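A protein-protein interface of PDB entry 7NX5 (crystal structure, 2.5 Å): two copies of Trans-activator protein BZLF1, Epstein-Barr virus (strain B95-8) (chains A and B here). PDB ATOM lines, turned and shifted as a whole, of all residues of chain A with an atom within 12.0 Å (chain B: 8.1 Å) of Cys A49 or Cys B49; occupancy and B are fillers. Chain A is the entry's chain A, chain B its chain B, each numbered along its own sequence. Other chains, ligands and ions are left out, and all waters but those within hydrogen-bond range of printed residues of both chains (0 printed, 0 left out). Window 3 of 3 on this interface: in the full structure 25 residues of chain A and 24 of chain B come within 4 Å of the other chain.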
ATOM      1  N   ARG A  40      -3.964 -21.396 -31.528  1.00  0.00           N
ATOM      2  CA  ARG A  40      -5.001 -22.102 -32.295  1.00  0.00           C
ATOM      3  C   ARG A  40      -6.310 -22.160 -31.516  1.00  0.00           C
ATOM      4  O   ARG A  40      -7.385 -21.801 -32.031  1.00  0.00           O
ATOM      5  CB  ARG A  40      -4.537 -23.510 -32.671  1.00  0.00           C
ATOM      6  CG  ARG A  40      -3.195 -23.538 -33.367  1.00  0.00           C
ATOM      7  CD  ARG A  40      -2.977 -24.850 -34.093  1.00  0.00           C
ATOM      8  NE  ARG A  40      -1.662 -24.941 -34.714  1.00  0.00           N
ATOM      9  CZ  ARG A  40      -1.437 -24.838 -36.027  1.00  0.00           C
ATOM     10  NH1 ARG A  40      -2.450 -24.631 -36.862  1.00  0.00           N
ATOM     11  NH2 ARG A  40      -0.198 -24.947 -36.516  1.00  0.00           N
ATOM     12  N   LEU A  41      -6.242 -22.604 -30.262  1.00  0.00           N
ATOM     13  CA  LEU A  41      -7.417 -22.704 -29.407  1.00  0.00           C
ATOM     14  C   LEU A  41      -8.114 -21.358 -29.268  1.00  0.00           C
ATOM     15  O   LEU A  41      -9.327 -21.253 -29.444  1.00  0.00           O
ATOM     16  CB  LEU A  41      -7.009 -23.232 -28.024  1.00  0.00           C
ATOM     17  CG  LEU A  41      -6.438 -24.652 -27.906  1.00  0.00           C
ATOM     18  CD1 LEU A  41      -5.819 -24.916 -26.527  1.00  0.00           C
ATOM     19  CD2 LEU A  41      -7.486 -25.690 -28.245  1.00  0.00           C
ATOM     20  N   ARG A  42      -7.353 -20.331 -28.909  1.00  0.00           N
ATOM     21  CA  ARG A  42      -7.926 -19.020 -28.621  1.00  0.00           C
ATOM     22  C   ARG A  42      -8.634 -18.460 -29.840  1.00  0.00           C
ATOM     23  O   ARG A  42      -9.710 -17.874 -29.726  1.00  0.00           O
ATOM     24  CB  ARG A  42      -6.817 -18.067 -28.158  1.00  0.00           C
ATOM     25  CG  ARG A  42      -7.268 -16.662 -27.823  1.00  0.00           C
ATOM     26  CD  ARG A  42      -6.106 -15.865 -27.250  1.00  0.00           C
ATOM     27  NE  ARG A  42      -5.492 -16.575 -26.130  1.00  0.00           N
ATOM     28  CZ  ARG A  42      -5.794 -16.373 -24.847  1.00  0.00           C
ATOM     29  NH1 ARG A  42      -6.691 -15.460 -24.509  1.00  0.00           N
ATOM     30  NH2 ARG A  42      -5.192 -17.088 -23.904  1.00  0.00           N
ATOM     31  N   LEU A  43      -8.038 -18.629 -31.024  1.00  0.00           N
ATOM     32  CA  LEU A  43      -8.657 -18.074 -32.214  1.00  0.00           C
ATOM     33  C   LEU A  43      -9.879 -18.872 -32.602  1.00  0.00           C
ATOM     34  O   LEU A  43     -10.867 -18.303 -33.068  1.00  0.00           O
ATOM     35  CB  LEU A  43      -7.668 -18.022 -33.373  1.00  0.00           C
ATOM     36  CG  LEU A  43      -7.022 -16.646 -33.573  1.00  0.00           C
ATOM     37  CD1 LEU A  43      -5.963 -16.418 -32.520  1.00  0.00           C
ATOM     38  CD2 LEU A  43      -6.454 -16.507 -34.978  1.00  0.00           C
ATOM     39  N   LEU A  44      -9.835 -20.187 -32.403  1.00  0.00           N
ATOM     40  CA  LEU A  44     -11.010 -20.996 -32.708  1.00  0.00           C
ATOM     41  C   LEU A  44     -12.181 -20.623 -31.807  1.00  0.00           C
ATOM     42  O   LEU A  44     -13.339 -20.580 -32.257  1.00  0.00           O
ATOM     43  CB  LEU A  44     -10.659 -22.471 -32.560  1.00  0.00           C
ATOM     44  CG  LEU A  44     -11.732 -23.528 -32.705  1.00  0.00           C
ATOM     45  CD1 LEU A  44     -12.049 -23.814 -34.181  1.00  0.00           C
ATOM     46  CD2 LEU A  44     -11.287 -24.763 -31.961  1.00  0.00           C
ATOM     47  N   LEU A  45     -11.899 -20.335 -30.531  1.00  0.00           N
ATOM     48  CA  LEU A  45     -12.969 -19.996 -29.601  1.00  0.00           C
ATOM     49  C   LEU A  45     -13.497 -18.592 -29.876  1.00  0.00           C
ATOM     50  O   LEU A  45     -14.713 -18.371 -29.879  1.00  0.00           O
ATOM     51  CB  LEU A  45     -12.471 -20.145 -28.163  1.00  0.00           C
ATOM     52  CG  LEU A  45     -13.380 -20.239 -26.937  1.00  0.00           C
ATOM     53  CD1 LEU A  45     -14.704 -20.915 -27.203  1.00  0.00           C
ATOM     54  CD2 LEU A  45     -12.647 -20.984 -25.842  1.00  0.00           C
ATOM     55  N   LYS A  46     -12.600 -17.635 -30.146  1.00  0.00           N
ATOM     56  CA  LYS A  46     -13.040 -16.318 -30.604  1.00  0.00           C
ATOM     57  C   LYS A  46     -13.921 -16.429 -31.842  1.00  0.00           C
ATOM     58  O   LYS A  46     -14.904 -15.693 -31.986  1.00  0.00           O
ATOM     59  CB  LYS A  46     -11.839 -15.425 -30.919  1.00  0.00           C
ATOM     60  CG  LYS A  46     -11.235 -14.716 -29.734  1.00  0.00           C
ATOM     61  CD  LYS A  46     -10.101 -13.814 -30.210  1.00  0.00           C
ATOM     62  CE  LYS A  46     -10.597 -12.842 -31.284  1.00  0.00           C
ATOM     63  NZ  LYS A  46      -9.635 -11.709 -31.561  1.00  0.00           N
ATOM     64  N   GLN A  47     -13.568 -17.336 -32.757  1.00  0.00           N
ATOM     65  CA  GLN A  47     -14.387 -17.566 -33.940  1.00  0.00           C
ATOM     66  C   GLN A  47     -15.763 -18.085 -33.554  1.00  0.00           C
ATOM     67  O   GLN A  47     -16.785 -17.587 -34.040  1.00  0.00           O
ATOM     68  CB  GLN A  47     -13.689 -18.558 -34.879  1.00  0.00           C
ATOM     69  CG  GLN A  47     -14.646 -19.570 -35.533  1.00  0.00           C
ATOM     70  CD  GLN A  47     -14.228 -19.979 -36.939  1.00  0.00           C
ATOM     71  OE1 GLN A  47     -13.041 -20.180 -37.220  1.00  0.00           O
ATOM     72  NE2 GLN A  47     -15.207 -20.091 -37.836  1.00  0.00           N
ATOM     73  N   MET A  48     -15.805 -19.084 -32.665  1.00  0.00           N
ATOM     74  CA  MET A  48     -17.032 -19.841 -32.431  1.00  0.00           C
ATOM     75  C   MET A  48     -17.998 -19.100 -31.523  1.00  0.00           C
ATOM     76  O   MET A  48     -19.203 -19.042 -31.807  1.00  0.00           O
ATOM     77  CB  MET A  48     -16.696 -21.203 -31.827  1.00  0.00           C
ATOM     78  CG  MET A  48     -15.892 -22.102 -32.734  1.00  0.00           C
ATOM     79  SD  MET A  48     -16.839 -22.431 -34.212  1.00  0.00           S
ATOM     80  CE  MET A  48     -17.637 -23.974 -33.740  1.00  0.00           C
ATOM     81  N   CYS A  49     -17.491 -18.543 -30.433  1.00  0.00           N
ATOM     82  CA  CYS A  49     -18.285 -17.792 -29.477  1.00  0.00           C
ATOM     83  C   CYS A  49     -17.844 -16.335 -29.505  1.00  0.00           C
ATOM     84  O   CYS A  49     -17.275 -15.843 -28.524  1.00  0.00           O
ATOM     85  CB  CYS A  49     -18.128 -18.383 -28.079  1.00  0.00           C
ATOM     86  SG  CYS A  49     -18.198 -20.186 -28.074  1.00  0.00           S
ATOM     87  N   PRO A  50     -18.110 -15.607 -30.599  1.00  0.00           N
ATOM     88  CA  PRO A  50     -17.522 -14.269 -30.754  1.00  0.00           C
ATOM     89  C   PRO A  50     -18.162 -13.235 -29.843  1.00  0.00           C
ATOM     90  O   PRO A  50     -17.853 -12.042 -29.940  1.00  0.00           O
ATOM     91  CB  PRO A  50     -17.772 -13.941 -32.233  1.00  0.00           C
ATOM     92  CG  PRO A  50     -18.413 -15.186 -32.837  1.00  0.00           C
ATOM     93  CD  PRO A  50     -19.033 -15.914 -31.698  1.00  0.00           C
ATOM     94  N   SER A  51     -19.052 -13.672 -28.955  1.00  0.00           N
ATOM     95  CA  SER A  51     -19.593 -12.780 -27.939  1.00  0.00           C
ATOM     96  C   SER A  51     -19.018 -13.143 -26.574  1.00  0.00           C
ATOM     97  O   SER A  51     -19.751 -13.255 -25.587  1.00  0.00           O
ATOM     98  N   LEU A  52     -17.704 -13.339 -26.503  1.00  0.00           N
ATOM     99  CA  LEU A  52     -17.033 -13.647 -25.247  1.00  0.00           C
ATOM    100  C   LEU A  52     -15.720 -12.885 -25.186  1.00  0.00           C
ATOM    101  O   LEU A  52     -15.005 -12.807 -26.185  1.00  0.00           O
ATOM    102  CB  LEU A  52     -16.769 -15.148 -25.108  1.00  0.00           C
ATOM    103  CG  LEU A  52     -16.381 -15.602 -23.703  1.00  0.00           C
ATOM    104  CD1 LEU A  52     -17.477 -15.225 -22.732  1.00  0.00           C
ATOM    105  CD2 LEU A  52     -16.123 -17.097 -23.661  1.00  0.00           C
ATOM    106  N   ASP A  53     -15.413 -12.327 -24.013  1.00  0.00           N
ATOM    107  CA  ASP A  53     -14.130 -11.667 -23.755  1.00  0.00           C
ATOM    108  C   ASP A  53     -13.073 -12.732 -23.461  1.00  0.00           C
ATOM    109  O   ASP A  53     -12.616 -12.908 -22.331  1.00  0.00           O
ATOM    110  CB  ASP A  53     -14.253 -10.693 -22.593  1.00  0.00           C
ATOM    111  CG  ASP A  53     -13.585  -9.367 -22.873  1.00  0.00           C
ATOM    112  OD1 ASP A  53     -12.698  -9.312 -23.750  1.00  0.00           O
ATOM    113  OD2 ASP A  53     -13.956  -8.371 -22.217  1.00  0.00           O
ATOM    114  N   VAL A  54     -12.685 -13.450 -24.521  1.00  0.00           N
ATOM    115  CA  VAL A  54     -11.779 -14.586 -24.363  1.00  0.00           C
ATOM    116  C   VAL A  54     -10.450 -14.128 -23.786  1.00  0.00           C
ATOM    117  O   VAL A  54      -9.994 -14.624 -22.748  1.00  0.00           O
ATOM    118  CB  VAL A  54     -11.579 -15.314 -25.703  1.00  0.00           C
ATOM    119  CG1 VAL A  54     -10.419 -16.284 -25.589  1.00  0.00           C
ATOM    120  CG2 VAL A  54     -12.851 -16.060 -26.101  1.00  0.00           C
ATOM    121  N   ASP A  55      -9.827 -13.146 -24.428  1.00  0.00           N
ATOM    122  CA  ASP A  55      -8.523 -12.654 -24.008  1.00  0.00           C
ATOM    123  C   ASP A  55      -8.607 -11.917 -22.673  1.00  0.00           C
ATOM    124  O   ASP A  55      -7.605 -11.392 -22.180  1.00  0.00           O
ATOM    125  CB  ASP A  55      -7.922 -11.757 -25.099  1.00  0.00           C
ATOM    126  CG  ASP A  55      -7.685 -12.505 -26.420  1.00  0.00           C
ATOM    127  OD1 ASP A  55      -8.174 -13.649 -26.564  1.00  0.00           O
ATOM    128  OD2 ASP A  55      -7.013 -11.943 -27.314  1.00  0.00           O
ATOM    129  N   SER A  56      -9.791 -11.882 -22.072  1.00  0.00           N
ATOM    130  CA  SER A  56      -9.968 -11.424 -20.700  1.00  0.00           C
ATOM    131  C   SER A  56     -10.316 -12.548 -19.737  1.00  0.00           C
ATOM    132  O   SER A  56      -9.797 -12.578 -18.617  1.00  0.00           O
ATOM    133  CB  SER A  56     -11.054 -10.344 -20.643  1.00  0.00           C
ATOM    134  OG  SER A  56     -10.637  -9.204 -21.378  1.00  0.00           O
ATOM    135  N   ILE A  57     -11.177 -13.481 -20.142  1.00  0.00           N
ATOM    136  CA  ILE A  57     -11.466 -14.614 -19.272  1.00  0.00           C
ATOM    137  C   ILE A  57     -10.242 -15.508 -19.149  1.00  0.00           C
ATOM    138  O   ILE A  57     -10.001 -16.099 -18.091  1.00  0.00           O
ATOM    139  CB  ILE A  57     -12.701 -15.394 -19.776  1.00  0.00           C
ATOM    140  CG1 ILE A  57     -13.016 -16.586 -18.866  1.00  0.00           C
ATOM    141  CG2 ILE A  57     -12.498 -15.881 -21.188  1.00  0.00           C
ATOM    142  CD1 ILE A  57     -13.571 -16.196 -17.512  1.00  0.00           C
ATOM    143  N   ILE A  58      -9.450 -15.628 -20.205  1.00  0.00           N
ATOM    144  CA  ILE A  58      -8.183 -16.344 -20.091  1.00  0.00           C
ATOM    145  C   ILE A  58      -7.086 -15.441 -20.633  1.00  0.00           C
ATOM    146  O   ILE A  58      -6.668 -15.590 -21.795  1.00  0.00           O
ATOM    147  CB  ILE A  58      -8.226 -17.696 -20.818  1.00  0.00           C
ATOM    148  CG1 ILE A  58      -9.602 -18.334 -20.680  1.00  0.00           C
ATOM    149  CG2 ILE A  58      -7.208 -18.632 -20.208  1.00  0.00           C
ATOM    150  CD1 ILE A  58      -9.869 -19.435 -21.659  1.00  0.00           C
ATOM    151  N   ARG B  42      -9.026 -25.544 -23.608  1.00  0.00           N
ATOM    152  CA  ARG B  42      -9.749 -26.743 -24.004  1.00  0.00           C
ATOM    153  C   ARG B  42     -11.032 -26.887 -23.185  1.00  0.00           C
ATOM    154  O   ARG B  42     -12.103 -27.117 -23.751  1.00  0.00           O
ATOM    155  CB  ARG B  42      -8.856 -27.975 -23.884  1.00  0.00           C
ATOM    156  CG  ARG B  42      -7.915 -28.131 -25.049  1.00  0.00           C
ATOM    157  CD  ARG B  42      -6.964 -29.341 -24.927  1.00  0.00           C
ATOM    158  NE  ARG B  42      -5.780 -29.248 -25.800  1.00  0.00           N
ATOM    159  CZ  ARG B  42      -5.811 -29.489 -27.098  1.00  0.00           C
ATOM    160  NH1 ARG B  42      -6.952 -29.849 -27.673  1.00  0.00           N
ATOM    161  NH2 ARG B  42      -4.716 -29.381 -27.826  1.00  0.00           N
ATOM    162  N   LEU B  43     -10.953 -26.698 -21.864  1.00  0.00           N
ATOM    163  CA  LEU B  43     -12.127 -26.727 -20.987  1.00  0.00           C
ATOM    164  C   LEU B  43     -13.241 -25.819 -21.481  1.00  0.00           C
ATOM    165  O   LEU B  43     -14.376 -26.258 -21.698  1.00  0.00           O
ATOM    166  CB  LEU B  43     -11.718 -26.283 -19.585  1.00  0.00           C
ATOM    167  CG  LEU B  43     -12.852 -26.296 -18.587  1.00  0.00           C
ATOM    168  CD1 LEU B  43     -13.228 -27.743 -18.327  1.00  0.00           C
ATOM    169  CD2 LEU B  43     -12.452 -25.561 -17.303  1.00  0.00           C
ATOM    170  N   LEU B  44     -12.947 -24.524 -21.589  1.00  0.00           N
ATOM    171  CA  LEU B  44     -13.969 -23.544 -21.921  1.00  0.00           C
ATOM    172  C   LEU B  44     -14.533 -23.762 -23.324  1.00  0.00           C
ATOM    173  O   LEU B  44     -15.718 -23.516 -23.557  1.00  0.00           O
ATOM    174  CB  LEU B  44     -13.403 -22.136 -21.784  1.00  0.00           C
ATOM    175  CG  LEU B  44     -14.456 -21.033 -21.825  1.00  0.00           C
ATOM    176  CD1 LEU B  44     -15.058 -20.952 -20.482  1.00  0.00           C
ATOM    177  CD2 LEU B  44     -13.845 -19.699 -22.270  1.00  0.00           C
ATOM    178  N   LEU B  45     -13.697 -24.172 -24.282  1.00  0.00           N
ATOM    179  CA  LEU B  45     -14.198 -24.599 -25.591  1.00  0.00           C
ATOM    180  C   LEU B  45     -15.098 -25.824 -25.510  1.00  0.00           C
ATOM    181  O   LEU B  45     -16.056 -25.947 -26.274  1.00  0.00           O
ATOM    182  CB  LEU B  45     -13.017 -24.861 -26.512  1.00  0.00           C
ATOM    183  CG  LEU B  45     -13.055 -25.026 -28.025  1.00  0.00           C
ATOM    184  CD1 LEU B  45     -14.005 -24.071 -28.722  1.00  0.00           C
ATOM    185  CD2 LEU B  45     -11.635 -24.702 -28.403  1.00  0.00           C
ATOM    186  N   LYS B  46     -14.810 -26.724 -24.596  1.00  0.00           N
ATOM    187  CA  LYS B  46     -15.649 -27.895 -24.408  1.00  0.00           C
ATOM    188  C   LYS B  46     -16.944 -27.547 -23.694  1.00  0.00           C
ATOM    189  O   LYS B  46     -17.901 -28.334 -23.706  1.00  0.00           O
ATOM    190  CB  LYS B  46     -14.865 -28.950 -23.622  1.00  0.00           C
ATOM    191  CG  LYS B  46     -15.677 -29.801 -22.688  1.00  0.00           C
ATOM    192  CD  LYS B  46     -14.822 -30.801 -21.917  1.00  0.00           C
ATOM    193  CE  LYS B  46     -13.917 -31.663 -22.791  1.00  0.00           C
ATOM    194  NZ  LYS B  46     -13.419 -32.882 -22.117  1.00  0.00           N
ATOM    195  N   GLN B  47     -16.995 -26.376 -23.059  1.00  0.00           N
ATOM    196  CA  GLN B  47     -18.241 -25.974 -22.406  1.00  0.00           C
ATOM    197  C   GLN B  47     -19.037 -24.980 -23.236  1.00  0.00           C
ATOM    198  O   GLN B  47     -20.260 -24.881 -23.078  1.00  0.00           O
ATOM    199  CB  GLN B  47     -17.992 -25.353 -21.027  1.00  0.00           C
ATOM    200  CG  GLN B  47     -17.229 -26.187 -20.040  1.00  0.00           C
ATOM    201  CD  GLN B  47     -16.601 -25.313 -19.005  1.00  0.00           C
ATOM    202  OE1 GLN B  47     -16.134 -24.218 -19.312  1.00  0.00           O
ATOM    203  NE2 GLN B  47     -16.603 -25.767 -17.769  1.00  0.00           N
ATOM    204  N   MET B  48     -18.371 -24.264 -24.130  1.00  0.00           N
ATOM    205  CA  MET B  48     -19.012 -23.316 -25.023  1.00  0.00           C
ATOM    206  C   MET B  48     -19.342 -23.904 -26.382  1.00  0.00           C
ATOM    207  O   MET B  48     -20.334 -23.493 -26.991  1.00  0.00           O
ATOM    208  CB  MET B  48     -18.110 -22.098 -25.214  1.00  0.00           C
ATOM    209  CG  MET B  48     -17.857 -21.350 -23.936  1.00  0.00           C
ATOM    210  SD  MET B  48     -19.365 -20.521 -23.486  1.00  0.00           S
ATOM    211  CE  MET B  48     -19.529 -19.495 -24.939  1.00  0.00           C
ATOM    212  N   CYS B  49     -18.512 -24.840 -26.870  1.00  0.00           N
ATOM    213  CA  CYS B  49     -18.762 -25.569 -28.115  1.00  0.00           C
ATOM    214  C   CYS B  49     -18.744 -27.067 -27.842  1.00  0.00           C
ATOM    215  O   CYS B  49     -18.060 -27.828 -28.528  1.00  0.00           O
ATOM    216  CB  CYS B  49     -17.709 -25.207 -29.152  1.00  0.00           C
ATOM    217  SG  CYS B  49     -17.396 -23.457 -29.295  1.00  0.00           S
ATOM    218  N   PRO B  50     -19.502 -27.528 -26.840  1.00  0.00           N
ATOM    219  CA  PRO B  50     -19.374 -28.933 -26.402  1.00  0.00           C
ATOM    220  C   PRO B  50     -19.519 -29.949 -27.523  1.00  0.00           C
ATOM    221  O   PRO B  50     -18.845 -30.988 -27.529  1.00  0.00           O
ATOM    222  CB  PRO B  50     -20.504 -29.070 -25.370  1.00  0.00           C
ATOM    223  CG  PRO B  50     -21.496 -28.034 -25.775  1.00  0.00           C
ATOM    224  CD  PRO B  50     -20.684 -26.878 -26.250  1.00  0.00           C
ATOM    225  N   SER B  51     -20.373 -29.656 -28.485  1.00  0.00           N
ATOM    226  CA  SER B  51     -20.692 -30.562 -29.576  1.00  0.00           C
ATOM    227  C   SER B  51     -19.612 -30.639 -30.620  1.00  0.00           C
ATOM    228  O   SER B  51     -19.927 -30.773 -31.805  1.00  0.00           O
ATOM    229  CB  SER B  51     -21.986 -30.076 -30.205  1.00  0.00           C
ATOM    230  N   LEU B  52     -18.344 -30.555 -30.222  1.00  0.00           N
ATOM    231  CA  LEU B  52     -17.265 -30.291 -31.161  1.00  0.00           C
ATOM    232  C   LEU B  52     -15.997 -30.981 -30.679  1.00  0.00           C
ATOM    233  O   LEU B  52     -15.730 -31.044 -29.475  1.00  0.00           O
ATOM    234  CB  LEU B  52     -17.046 -28.776 -31.307  1.00  0.00           C
ATOM    235  CG  LEU B  52     -16.183 -28.219 -32.443  1.00  0.00           C
ATOM    236  N   ASP B  53     -15.207 -31.484 -31.631  1.00  0.00           N
ATOM    237  CA  ASP B  53     -14.017 -32.269 -31.320  1.00  0.00           C
ATOM    238  C   ASP B  53     -12.771 -31.398 -31.458  1.00  0.00           C
ATOM    239  O   ASP B  53     -12.379 -31.020 -32.568  1.00  0.00           O
ATOM    240  CB  ASP B  53     -13.919 -33.514 -32.198  1.00  0.00           C
ATOM    241  CG  ASP B  53     -12.858 -34.481 -31.699  1.00  0.00           C
ATOM    242  OD1 ASP B  53     -12.134 -34.132 -30.726  1.00  0.00           O
ATOM    243  OD2 ASP B  53     -12.747 -35.587 -32.267  1.00  0.00           O
ATOM    244  N   VAL B  54     -12.145 -31.111 -30.316  1.00  0.00           N
ATOM    245  CA  VAL B  54     -10.961 -30.263 -30.257  1.00  0.00           C
ATOM    246  C   VAL B  54      -9.682 -31.094 -30.338  1.00  0.00           C
ATOM    247  O   VAL B  54      -8.621 -30.563 -30.697  1.00  0.00           O
ATOM    248  CB  VAL B  54     -11.015 -29.407 -28.972  1.00  0.00           C
ATOM    249  CG1 VAL B  54      -9.792 -28.558 -28.815  1.00  0.00           C
ATOM    250  CG2 VAL B  54     -12.282 -28.520 -28.937  1.00  0.00           C
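SG of Cys A49 lies within hydrogen-bond range of SG of Cys B49 (3.6 Å).
Among the printed residues, pairs that only touch across the chains: Cys A49 with Met B48 (3.4 Å), Met A48 with Cys B49 (3.5 Å), Leu A45 with Leu B45 (3.6 Å), Leu A44 with Leu B45 (3.6 Å), Leu A41 with Val B54 (3.7 Å), Leu A52 with Leu B44 (3.7 Å) and Leu A45 with Leu B44 (3.98 Å).
Of the printed residues of chain B, Leu A44 touches Leu B45 (3.6 Å). Printed residues of chain B within 4 Å of Leu A45: Leu B44 and Leu B45. Of the printed residues of chain B, Met A48 touches Cys B49. Cys A49 touches just these residues of chain B: Met B48 (3.4 Å) and Cys B49 (3.6 Å). Of the printed residues of chain B, Leu A52 touches Leu B44. Leu B43 touches none of the printed residues of chain A. Pro B50 touches none of the printed residues of chain A. No residue of chain A comes within 4 Å of Ser B51. No residue of chain A comes within 4 Å of Leu B52. Of the printed residues of chain A, Val B54 touches Leu A41 (3.7 Å). The nearest residue of chain B that does not touch Cys A49 is Leu B45 (5.8 Å).
Of the 19 printed residues of chain A, 6 touch a printed residue of chain B. Printed residues of chain A that touch a printed residue of chain B: Leu A41, Leu A44, Leu A45, Met A48, Cys A49 and Leu A52. Hydrophobic or aromatic side chains of chain A within 4 Å of the printed part of chain B: Leu A41, Leu A44, Leu A45, Met A48 and Leu A52. Along chain B the printed residues that touch a printed residue of chain A span positions 44 to 54. Among the printed residues, 8 pairs touch across the chains. Among the printed residues, no Asp or Glu carboxylate lies within 4 Å of a Lys or Arg side-chain nitrogen of the other chain.
Leu A44 touches Leu B45, and with the chains exchanged Leu A45 touches Leu B44. Met A48 touches Cys B49, and with the chains exchanged Cys A49 touches Met B48. Cys A49 touches its own counterpart, Cys B49. Leu A52 touches Leu B44, but with the chains exchanged Leu A44 does not touch Leu B52 (6.0 Å).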
